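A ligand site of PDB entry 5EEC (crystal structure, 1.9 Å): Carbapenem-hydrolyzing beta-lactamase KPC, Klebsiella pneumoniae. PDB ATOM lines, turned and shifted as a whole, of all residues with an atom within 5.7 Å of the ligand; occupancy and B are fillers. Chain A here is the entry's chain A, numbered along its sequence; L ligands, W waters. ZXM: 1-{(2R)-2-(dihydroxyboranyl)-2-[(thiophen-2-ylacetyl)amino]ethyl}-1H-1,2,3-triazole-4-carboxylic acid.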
ATOM      1  N   LEU A  43       0.809  -7.074  13.785  1.00  0.00           N
ATOM      2  CA  LEU A  43      -0.335  -6.839  14.676  1.00  0.00           C
ATOM      3  C   LEU A  43      -0.170  -5.647  15.616  1.00  0.00           C
ATOM      4  O   LEU A  43      -1.139  -4.937  15.939  1.00  0.00           O
ATOM      5  CB  LEU A  43      -0.592  -8.107  15.471  1.00  0.00           C
ATOM      6  CG  LEU A  43      -1.023  -9.267  14.587  1.00  0.00           C
ATOM      7  CD1 LEU A  43      -0.766 -10.624  15.239  1.00  0.00           C
ATOM      8  CD2 LEU A  43      -2.511  -9.045  14.297  1.00  0.00           C
ATOM      9  N   CYS A  44       1.066  -5.448  16.054  1.00  0.00           N
ATOM     10  CA  CYS A  44       1.370  -4.550  17.157  1.00  0.00           C
ATOM     11  C   CYS A  44       0.363  -4.898  18.227  1.00  0.00           C
ATOM     12  O   CYS A  44       0.063  -6.102  18.422  1.00  0.00           O
ATOM     13  CB  CYS A  44       1.291  -3.079  16.728  1.00  0.00           C
ATOM     14  SG  CYS A  44       2.076  -2.684  15.149  1.00  0.00           S
ATOM     15  N   SER A  45      -0.216  -3.896  18.900  1.00  0.00           N
ATOM     16  CA  SER A  45      -1.090  -4.182  20.054  1.00  0.00           C
ATOM     17  C   SER A  45      -2.485  -4.719  19.703  1.00  0.00           C
ATOM     18  O   SER A  45      -3.271  -5.038  20.597  1.00  0.00           O
ATOM     19  CB  SER A  45      -1.250  -2.952  20.947  1.00  0.00           C
ATOM     20  OG  SER A  45      -0.082  -2.741  21.744  1.00  0.00           O
ATOM     21  N   SER A  46      -2.823  -4.738  18.420  1.00  0.00           N
ATOM     22  CA  SER A  46      -4.126  -5.235  18.009  1.00  0.00           C
ATOM     23  C   SER A  46      -4.322  -6.724  18.333  1.00  0.00           C
ATOM     24  O   SER A  46      -5.428  -7.194  18.345  1.00  0.00           O
ATOM     25  CB  SER A  46      -4.376  -4.968  16.521  1.00  0.00           C
ATOM     26  OG  SER A  46      -3.653  -5.830  15.667  1.00  0.00           O
ATOM     27  N   PHE A  47      -3.251  -7.468  18.600  1.00  0.00           N
ATOM     28  CA  PHE A  47      -3.397  -8.843  19.072  1.00  0.00           C
ATOM     29  C   PHE A  47      -4.172  -8.924  20.396  1.00  0.00           C
ATOM     30  O   PHE A  47      -4.774  -9.951  20.695  1.00  0.00           O
ATOM     31  CB  PHE A  47      -2.053  -9.553  19.246  1.00  0.00           C
ATOM     32  CG  PHE A  47      -1.390  -9.320  20.557  1.00  0.00           C
ATOM     33  CD1 PHE A  47      -1.614 -10.173  21.625  1.00  0.00           C
ATOM     34  CD2 PHE A  47      -0.510  -8.244  20.717  1.00  0.00           C
ATOM     35  CE1 PHE A  47      -0.949  -9.974  22.838  1.00  0.00           C
ATOM     36  CE2 PHE A  47       0.147  -8.035  21.911  1.00  0.00           C
ATOM     37  CZ  PHE A  47      -0.112  -8.885  22.990  1.00  0.00           C
ATOM     38  N   LYS A  48      -4.175  -7.836  21.180  1.00  0.00           N
ATOM     39  CA  LYS A  48      -4.815  -7.864  22.507  1.00  0.00           C
ATOM     40  C   LYS A  48      -6.313  -8.070  22.454  1.00  0.00           C
ATOM     41  O   LYS A  48      -6.891  -8.620  23.403  1.00  0.00           O
ATOM     42  CB  LYS A  48      -4.478  -6.613  23.310  1.00  0.00           C
ATOM     43  CG  LYS A  48      -2.971  -6.495  23.597  1.00  0.00           C
ATOM     44  CD  LYS A  48      -2.562  -5.094  24.010  1.00  0.00           C
ATOM     45  CE  LYS A  48      -1.063  -5.055  24.277  1.00  0.00           C
ATOM     46  NZ  LYS A  48      -0.542  -3.653  24.395  1.00  0.00           N
ATOM     47  N   PRO A  79       6.762  -0.662  29.928  1.00  0.00           N
ATOM     48  CA  PRO A  79       6.186   0.600  29.394  1.00  0.00           C
ATOM     49  C   PRO A  79       4.832   0.381  28.744  1.00  0.00           C
ATOM     50  O   PRO A  79       4.471  -0.755  28.401  1.00  0.00           O
ATOM     51  CB  PRO A  79       7.185   1.041  28.352  1.00  0.00           C
ATOM     52  CG  PRO A  79       8.452   0.351  28.753  1.00  0.00           C
ATOM     53  CD  PRO A  79       8.081  -0.939  29.359  1.00  0.00           C
ATOM     54  N   TRP A  80       4.097   1.463  28.594  1.00  0.00           N
ATOM     55  CA  TRP A  80       2.773   1.422  28.037  1.00  0.00           C
ATOM     56  C   TRP A  80       1.840   0.510  28.837  1.00  0.00           C
ATOM     57  O   TRP A  80       1.093  -0.292  28.271  1.00  0.00           O
ATOM     58  CB  TRP A  80       2.835   1.055  26.551  1.00  0.00           C
ATOM     59  CG  TRP A  80       2.573   2.247  25.743  1.00  0.00           C
ATOM     60  CD1 TRP A  80       3.488   3.096  25.179  1.00  0.00           C
ATOM     61  CD2 TRP A  80       1.286   2.783  25.465  1.00  0.00           C
ATOM     62  NE1 TRP A  80       2.837   4.124  24.532  1.00  0.00           N
ATOM     63  CE2 TRP A  80       1.480   3.967  24.701  1.00  0.00           C
ATOM     64  CE3 TRP A  80      -0.018   2.370  25.766  1.00  0.00           C
ATOM     65  CZ2 TRP A  80       0.409   4.725  24.223  1.00  0.00           C
ATOM     66  CZ3 TRP A  80      -1.078   3.136  25.282  1.00  0.00           C
ATOM     67  CH2 TRP A  80      -0.854   4.306  24.537  1.00  0.00           C
ATOM     68  N   TYR A 104      -7.244   0.046  26.974  1.00  0.00           N
ATOM     69  CA  TYR A 104      -6.099   0.940  27.170  1.00  0.00           C
ATOM     70  C   TYR A 104      -4.845   0.431  26.528  1.00  0.00           C
ATOM     71  O   TYR A 104      -3.818   1.048  26.648  1.00  0.00           O
ATOM     72  CB  TYR A 104      -5.877   1.211  28.668  1.00  0.00           C
ATOM     73  CG  TYR A 104      -7.004   2.060  29.221  1.00  0.00           C
ATOM     74  CD1 TYR A 104      -6.924   3.462  29.241  1.00  0.00           C
ATOM     75  CD2 TYR A 104      -8.178   1.464  29.665  1.00  0.00           C
ATOM     76  CE1 TYR A 104      -7.979   4.220  29.724  1.00  0.00           C
ATOM     77  CE2 TYR A 104      -9.227   2.206  30.138  1.00  0.00           C
ATOM     78  CZ  TYR A 104      -9.115   3.575  30.188  1.00  0.00           C
ATOM     79  OH  TYR A 104     -10.215   4.258  30.663  1.00  0.00           O
ATOM     80  N   SER A 105      -4.935  -0.701  25.849  1.00  0.00           N
ATOM     81  CA  SER A 105      -3.784  -1.314  25.207  1.00  0.00           C
ATOM     82  C   SER A 105      -2.636  -1.622  26.199  1.00  0.00           C
ATOM     83  O   SER A 105      -1.431  -1.501  25.839  1.00  0.00           O
ATOM     84  CB  SER A 105      -3.297  -0.403  24.098  1.00  0.00           C
ATOM     85  OG  SER A 105      -2.922  -1.176  23.011  1.00  0.00           O
ATOM     86  N   ASN A 107       0.193  -3.099  28.221  1.00  0.00           N
ATOM     87  CA  ASN A 107       1.182  -4.128  27.895  1.00  0.00           C
ATOM     88  C   ASN A 107       1.353  -5.172  28.958  1.00  0.00           C
ATOM     89  O   ASN A 107       1.330  -6.377  28.677  1.00  0.00           O
ATOM     90  CB  ASN A 107       2.567  -3.518  27.558  1.00  0.00           C
ATOM     91  CG  ASN A 107       2.685  -3.054  26.114  1.00  0.00           C
ATOM     92  OD1 ASN A 107       2.008  -3.552  25.230  1.00  0.00           O
ATOM     93  ND2 ASN A 107       3.565  -2.069  25.877  1.00  0.00           N
ATOM     94  N   GLU A 141       5.004  -8.719  24.438  1.00  0.00           N
ATOM     95  CA  GLU A 141       5.274  -7.299  24.565  1.00  0.00           C
ATOM     96  C   GLU A 141       6.630  -7.181  25.255  1.00  0.00           C
ATOM     97  O   GLU A 141       6.860  -7.912  26.189  1.00  0.00           O
ATOM     98  CB  GLU A 141       4.173  -6.578  25.363  1.00  0.00           C
ATOM     99  CG  GLU A 141       2.870  -6.429  24.610  1.00  0.00           C
ATOM    100  CD  GLU A 141       2.958  -5.460  23.436  1.00  0.00           C
ATOM    101  OE1 GLU A 141       4.054  -4.902  23.153  1.00  0.00           O
ATOM    102  OE2 GLU A 141       1.908  -5.291  22.750  1.00  0.00           O
ATOM    103  N   LEU A 142       7.552  -6.320  24.811  1.00  0.00           N
ATOM    104  CA  LEU A 142       7.375  -5.316  23.768  1.00  0.00           C
ATOM    105  C   LEU A 142       7.989  -5.696  22.408  1.00  0.00           C
ATOM    106  O   LEU A 142       7.841  -4.958  21.438  1.00  0.00           O
ATOM    107  CB  LEU A 142       8.083  -4.025  24.185  1.00  0.00           C
ATOM    108  CG  LEU A 142       7.686  -3.151  25.391  1.00  0.00           C
ATOM    109  CD1 LEU A 142       7.070  -1.831  24.918  1.00  0.00           C
ATOM    110  CD2 LEU A 142       6.820  -3.798  26.424  1.00  0.00           C
ATOM    111  N   LEU A 144       7.471  -7.889  20.126  1.00  0.00           N
ATOM    112  CA  LEU A 144       6.501  -8.094  19.023  1.00  0.00           C
ATOM    113  C   LEU A 144       6.231  -6.862  18.170  1.00  0.00           C
ATOM    114  O   LEU A 144       5.627  -6.971  17.089  1.00  0.00           O
ATOM    115  CB  LEU A 144       5.164  -8.671  19.549  1.00  0.00           C
ATOM    116  CG  LEU A 144       4.254  -7.869  20.475  1.00  0.00           C
ATOM    117  CD1 LEU A 144       3.456  -6.795  19.746  1.00  0.00           C
ATOM    118  CD2 LEU A 144       3.307  -8.835  21.174  1.00  0.00           C
ATOM    119  N   ASN A 145       6.700  -5.708  18.647  1.00  0.00           N
ATOM    120  CA  ASN A 145       6.526  -4.446  17.961  1.00  0.00           C
ATOM    121  C   ASN A 145       7.644  -4.089  16.983  1.00  0.00           C
ATOM    122  O   ASN A 145       7.644  -2.965  16.439  1.00  0.00           O
ATOM    123  CB  ASN A 145       6.463  -3.296  18.956  1.00  0.00           C
ATOM    124  CG  ASN A 145       5.220  -3.308  19.796  1.00  0.00           C
ATOM    125  OD1 ASN A 145       4.090  -3.157  19.298  1.00  0.00           O
ATOM    126  ND2 ASN A 145       5.415  -3.408  21.076  1.00  0.00           N
ATOM    127  N   ARG A 195      -9.146   6.868  14.577  1.00  0.00           N
ATOM    128  CA  ARG A 195      -8.867   5.843  13.620  1.00  0.00           C
ATOM    129  C   ARG A 195     -10.187   5.470  13.012  1.00  0.00           C
ATOM    130  O   ARG A 195     -10.837   6.360  12.477  1.00  0.00           O
ATOM    131  CB  ARG A 195      -8.088   4.707  14.316  1.00  0.00           C
ATOM    132  CG  ARG A 195      -6.753   5.204  14.767  1.00  0.00           C
ATOM    133  CD  ARG A 195      -5.754   4.122  15.192  1.00  0.00           C
ATOM    134  NE  ARG A 195      -4.564   4.749  15.757  1.00  0.00           N
ATOM    135  CZ  ARG A 195      -3.427   4.129  16.070  1.00  0.00           C
ATOM    136  NH1 ARG A 195      -3.285   2.819  15.857  1.00  0.00           N
ATOM    137  NH2 ARG A 195      -2.408   4.826  16.579  1.00  0.00           N
ATOM    138  N   LYS A 209     -10.290  -2.262  18.197  1.00  0.00           N
ATOM    139  CA  LYS A 209      -9.002  -2.418  18.857  1.00  0.00           C
ATOM    140  C   LYS A 209      -7.855  -1.856  17.991  1.00  0.00           C
ATOM    141  O   LYS A 209      -7.676  -2.245  16.835  1.00  0.00           O
ATOM    142  CB  LYS A 209      -8.721  -3.894  19.169  1.00  0.00           C
ATOM    143  CG  LYS A 209      -7.349  -4.145  19.832  1.00  0.00           C
ATOM    144  CD  LYS A 209      -7.334  -3.668  21.257  1.00  0.00           C
ATOM    145  CE  LYS A 209      -5.958  -3.535  21.861  1.00  0.00           C
ATOM    146  NZ  LYS A 209      -5.358  -2.188  21.652  1.00  0.00           N
ATOM    147  N   THR A 210      -7.032  -0.981  18.569  1.00  0.00           N
ATOM    148  CA  THR A 210      -5.888  -0.390  17.846  1.00  0.00           C
ATOM    149  C   THR A 210      -4.581  -1.133  18.066  1.00  0.00           C
ATOM    150  O   THR A 210      -4.460  -2.001  18.929  1.00  0.00           O
ATOM    151  CB  THR A 210      -5.654   1.047  18.327  1.00  0.00           C
ATOM    152  OG1 THR A 210      -5.377   1.057  19.720  1.00  0.00           O
ATOM    153  CG2 THR A 210      -6.900   1.915  18.091  1.00  0.00           C
ATOM    154  N   GLY A 211      -3.599  -0.806  17.261  1.00  0.00           N
ATOM    155  CA  GLY A 211      -2.247  -1.247  17.454  1.00  0.00           C
ATOM    156  C   GLY A 211      -1.289  -0.168  16.972  1.00  0.00           C
ATOM    157  O   GLY A 211      -1.577   0.518  15.974  1.00  0.00           O
ATOM    158  N   THR A 212      -0.188  -0.004  17.703  1.00  0.00           N
ATOM    159  CA  THR A 212       0.817   0.972  17.289  1.00  0.00           C
ATOM    160  C   THR A 212       2.194   0.403  17.652  1.00  0.00           C
ATOM    161  O   THR A 212       2.526   0.175  18.845  1.00  0.00           O
ATOM    162  CB  THR A 212       0.624   2.314  17.975  1.00  0.00           C
ATOM    163  OG1 THR A 212      -0.738   2.774  17.843  1.00  0.00           O
ATOM    164  CG2 THR A 212       1.595   3.361  17.434  1.00  0.00           C
ATOM    165  N   CYS A 213       2.990   0.125  16.631  1.00  0.00           N
ATOM    166  CA  CYS A 213       4.265  -0.539  16.903  1.00  0.00           C
ATOM    167  C   CYS A 213       5.281   0.500  17.372  1.00  0.00           C
ATOM    168  O   CYS A 213       6.169   0.191  18.150  1.00  0.00           O
ATOM    169  CB  CYS A 213       4.763  -1.295  15.657  1.00  0.00           C
ATOM    170  SG  CYS A 213       4.077  -2.960  15.470  1.00  0.00           S
ATOM    171  N   GLY A 214       5.123   1.740  16.918  1.00  0.00           N
ATOM    172  CA  GLY A 214       6.046   2.820  17.270  1.00  0.00           C
ATOM    173  C   GLY A 214       7.315   2.909  16.427  1.00  0.00           C
ATOM    174  O   GLY A 214       8.200   3.650  16.768  1.00  0.00           O
ATOM    175  N   HIS A 248       3.978   6.801  11.877  1.00  0.00           N
ATOM    176  CA  HIS A 248       2.658   6.302  11.610  1.00  0.00           C
ATOM    177  C   HIS A 248       1.731   7.478  11.543  1.00  0.00           C
ATOM    178  O   HIS A 248       2.111   8.568  11.929  1.00  0.00           O
ATOM    179  CB  HIS A 248       2.211   5.276  12.667  1.00  0.00           C
ATOM    180  CG  HIS A 248       1.826   5.868  13.982  1.00  0.00           C
ATOM    181  ND1 HIS A 248       2.752   6.198  14.947  1.00  0.00           N
ATOM    182  CD2 HIS A 248       0.615   6.202  14.492  1.00  0.00           C
ATOM    183  CE1 HIS A 248       2.121   6.681  16.009  1.00  0.00           C
ATOM    184  NE2 HIS A 248       0.821   6.692  15.750  1.00  0.00           N
HETATM  185  B1  ZXM L   1       1.291  -2.281  21.225  1.00  0.00           B
HETATM  186  O1  ZXM L   1       1.938  -3.625  20.858  1.00  0.00           O
HETATM  187  O2  ZXM L   1       0.913  -1.527  19.957  1.00  0.00           O
HETATM  188  N4  ZXM L   1       0.765   0.712  22.543  1.00  0.00           N
HETATM  189  N5  ZXM L   1      -0.588   0.733  22.199  1.00  0.00           N
HETATM  190  N6  ZXM L   1      -0.896   1.835  21.593  1.00  0.00           N
HETATM  191  C7  ZXM L   1       2.155  -1.446  22.308  1.00  0.00           C
HETATM  192  C8  ZXM L   1       1.316  -0.486  23.193  1.00  0.00           C
HETATM  193  N10 ZXM L   1       3.229  -0.785  21.591  1.00  0.00           N
HETATM  194  C11 ZXM L   1       4.381  -0.525  22.248  1.00  0.00           C
HETATM  195  C12 ZXM L   1       5.462   0.073  21.400  1.00  0.00           C
HETATM  196  C13 ZXM L   1       5.283   1.558  21.290  1.00  0.00           C
HETATM  197  C14 ZXM L   1       4.511   2.404  20.501  1.00  0.00           C
HETATM  198  C15 ZXM L   1       4.699   3.763  20.822  1.00  0.00           C
HETATM  199  C16 ZXM L   1       5.630   3.958  21.840  1.00  0.00           C
HETATM  200  O18 ZXM L   1       4.556  -0.745  23.466  1.00  0.00           O
HETATM  201  C19 ZXM L   1       0.226   2.602  21.548  1.00  0.00           C
HETATM  202  C20 ZXM L   1       1.274   1.868  22.127  1.00  0.00           C
HETATM  203  C21 ZXM L   1       0.374   3.968  20.995  1.00  0.00           C
HETATM  204  O22 ZXM L   1       1.486   4.453  20.871  1.00  0.00           O
HETATM  205  O23 ZXM L   1      -0.622   4.620  20.684  1.00  0.00           O
HETATM  206  S24 ZXM L   1       6.243   2.452  22.439  1.00  0.00           S
HETATM  207  O   HOH W   1       3.615   6.381  23.105  1.00  0.00           O
HETATM  208  O   HOH W   2      -2.513   1.926  19.422  1.00  0.00           O
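The side-chain hydroxyl (OG) of Ser 105 lies within hydrogen-bond range of a nitrogen (N5) of the ligand, 3.1 Å away.
OG of Ser 45 is covalently linked to B1 of the ligand.
O1 of the ligand is in hydrogen-bond range of OD1 of Asn 145.
N of Thr 212 lies within hydrogen-bond range of O2 of the ligand.
O1 of the ligand is in hydrogen-bond range of OE2 of Glu 141, at 2.5 Å.
The backbone carbonyl oxygen (O) of Thr 212 lies within hydrogen-bond range of an oxygen (O2) of the ligand (2.6 Å).
The side-chain hydroxyl of Thr 212 is in hydrogen-bond range of an oxygen (O23) of the ligand, at 3.4 Å.
An oxygen (O18) of the ligand lies within hydrogen-bond range of the side-chain amide nitrogen (ND2) of Asn 107 (2.9 Å).
The backbone NH (N) of Ser 45 lies close to an oxygen (O2) of the ligand (2.8 Å).
The side-chain amino group of Lys 48 is in hydrogen-bond range of the side-chain hydroxyl of Ser 45, at 2.8 Å.
OE2 of Glu 141 sits close to OD1 of Asn 107.
OE1 of Glu 141 lies within hydrogen-bond range of ND2 of Asn 145 (2.9 Å).
OG of Ser 45 lies close to OG of Ser 105.
SG of Cys 213 forms a disulfide with SG of Cys 44 (2.0 Å).
NZ of Lys 48 lies within salt-bridge range of OE2 of Glu 141, at 3.4 Å.
ND2 of Asn 107 sits at hydrogen-bond distance from O of Pro 79 (3.0 Å).
The side-chain hydroxyl of Thr 212 is in hydrogen-bond range of the guanidinium group of Arg 195, 2.9 Å away.
Merely in contact with the ligand: Leu 142 (3.1 Å), Trp 80 (3.3 Å), Cys 44 (3.3 Å), Cys 213 (3.3 Å), Gly 214 (3.6 Å), Leu 144 (3.7 Å), Lys 48 (3.9 Å) and Gly 211 (3.95 Å).
Hydrophobic or aromatic side chains within 4 Å of the ligand: Trp 80, Leu 142 and Leu 144.
Water W2 lies within hydrogen-bond range of OG1 of Thr 212 (2.5 Å), N6 of the ligand (2.7 Å) and OG1 of Thr 210 (3.0 Å).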
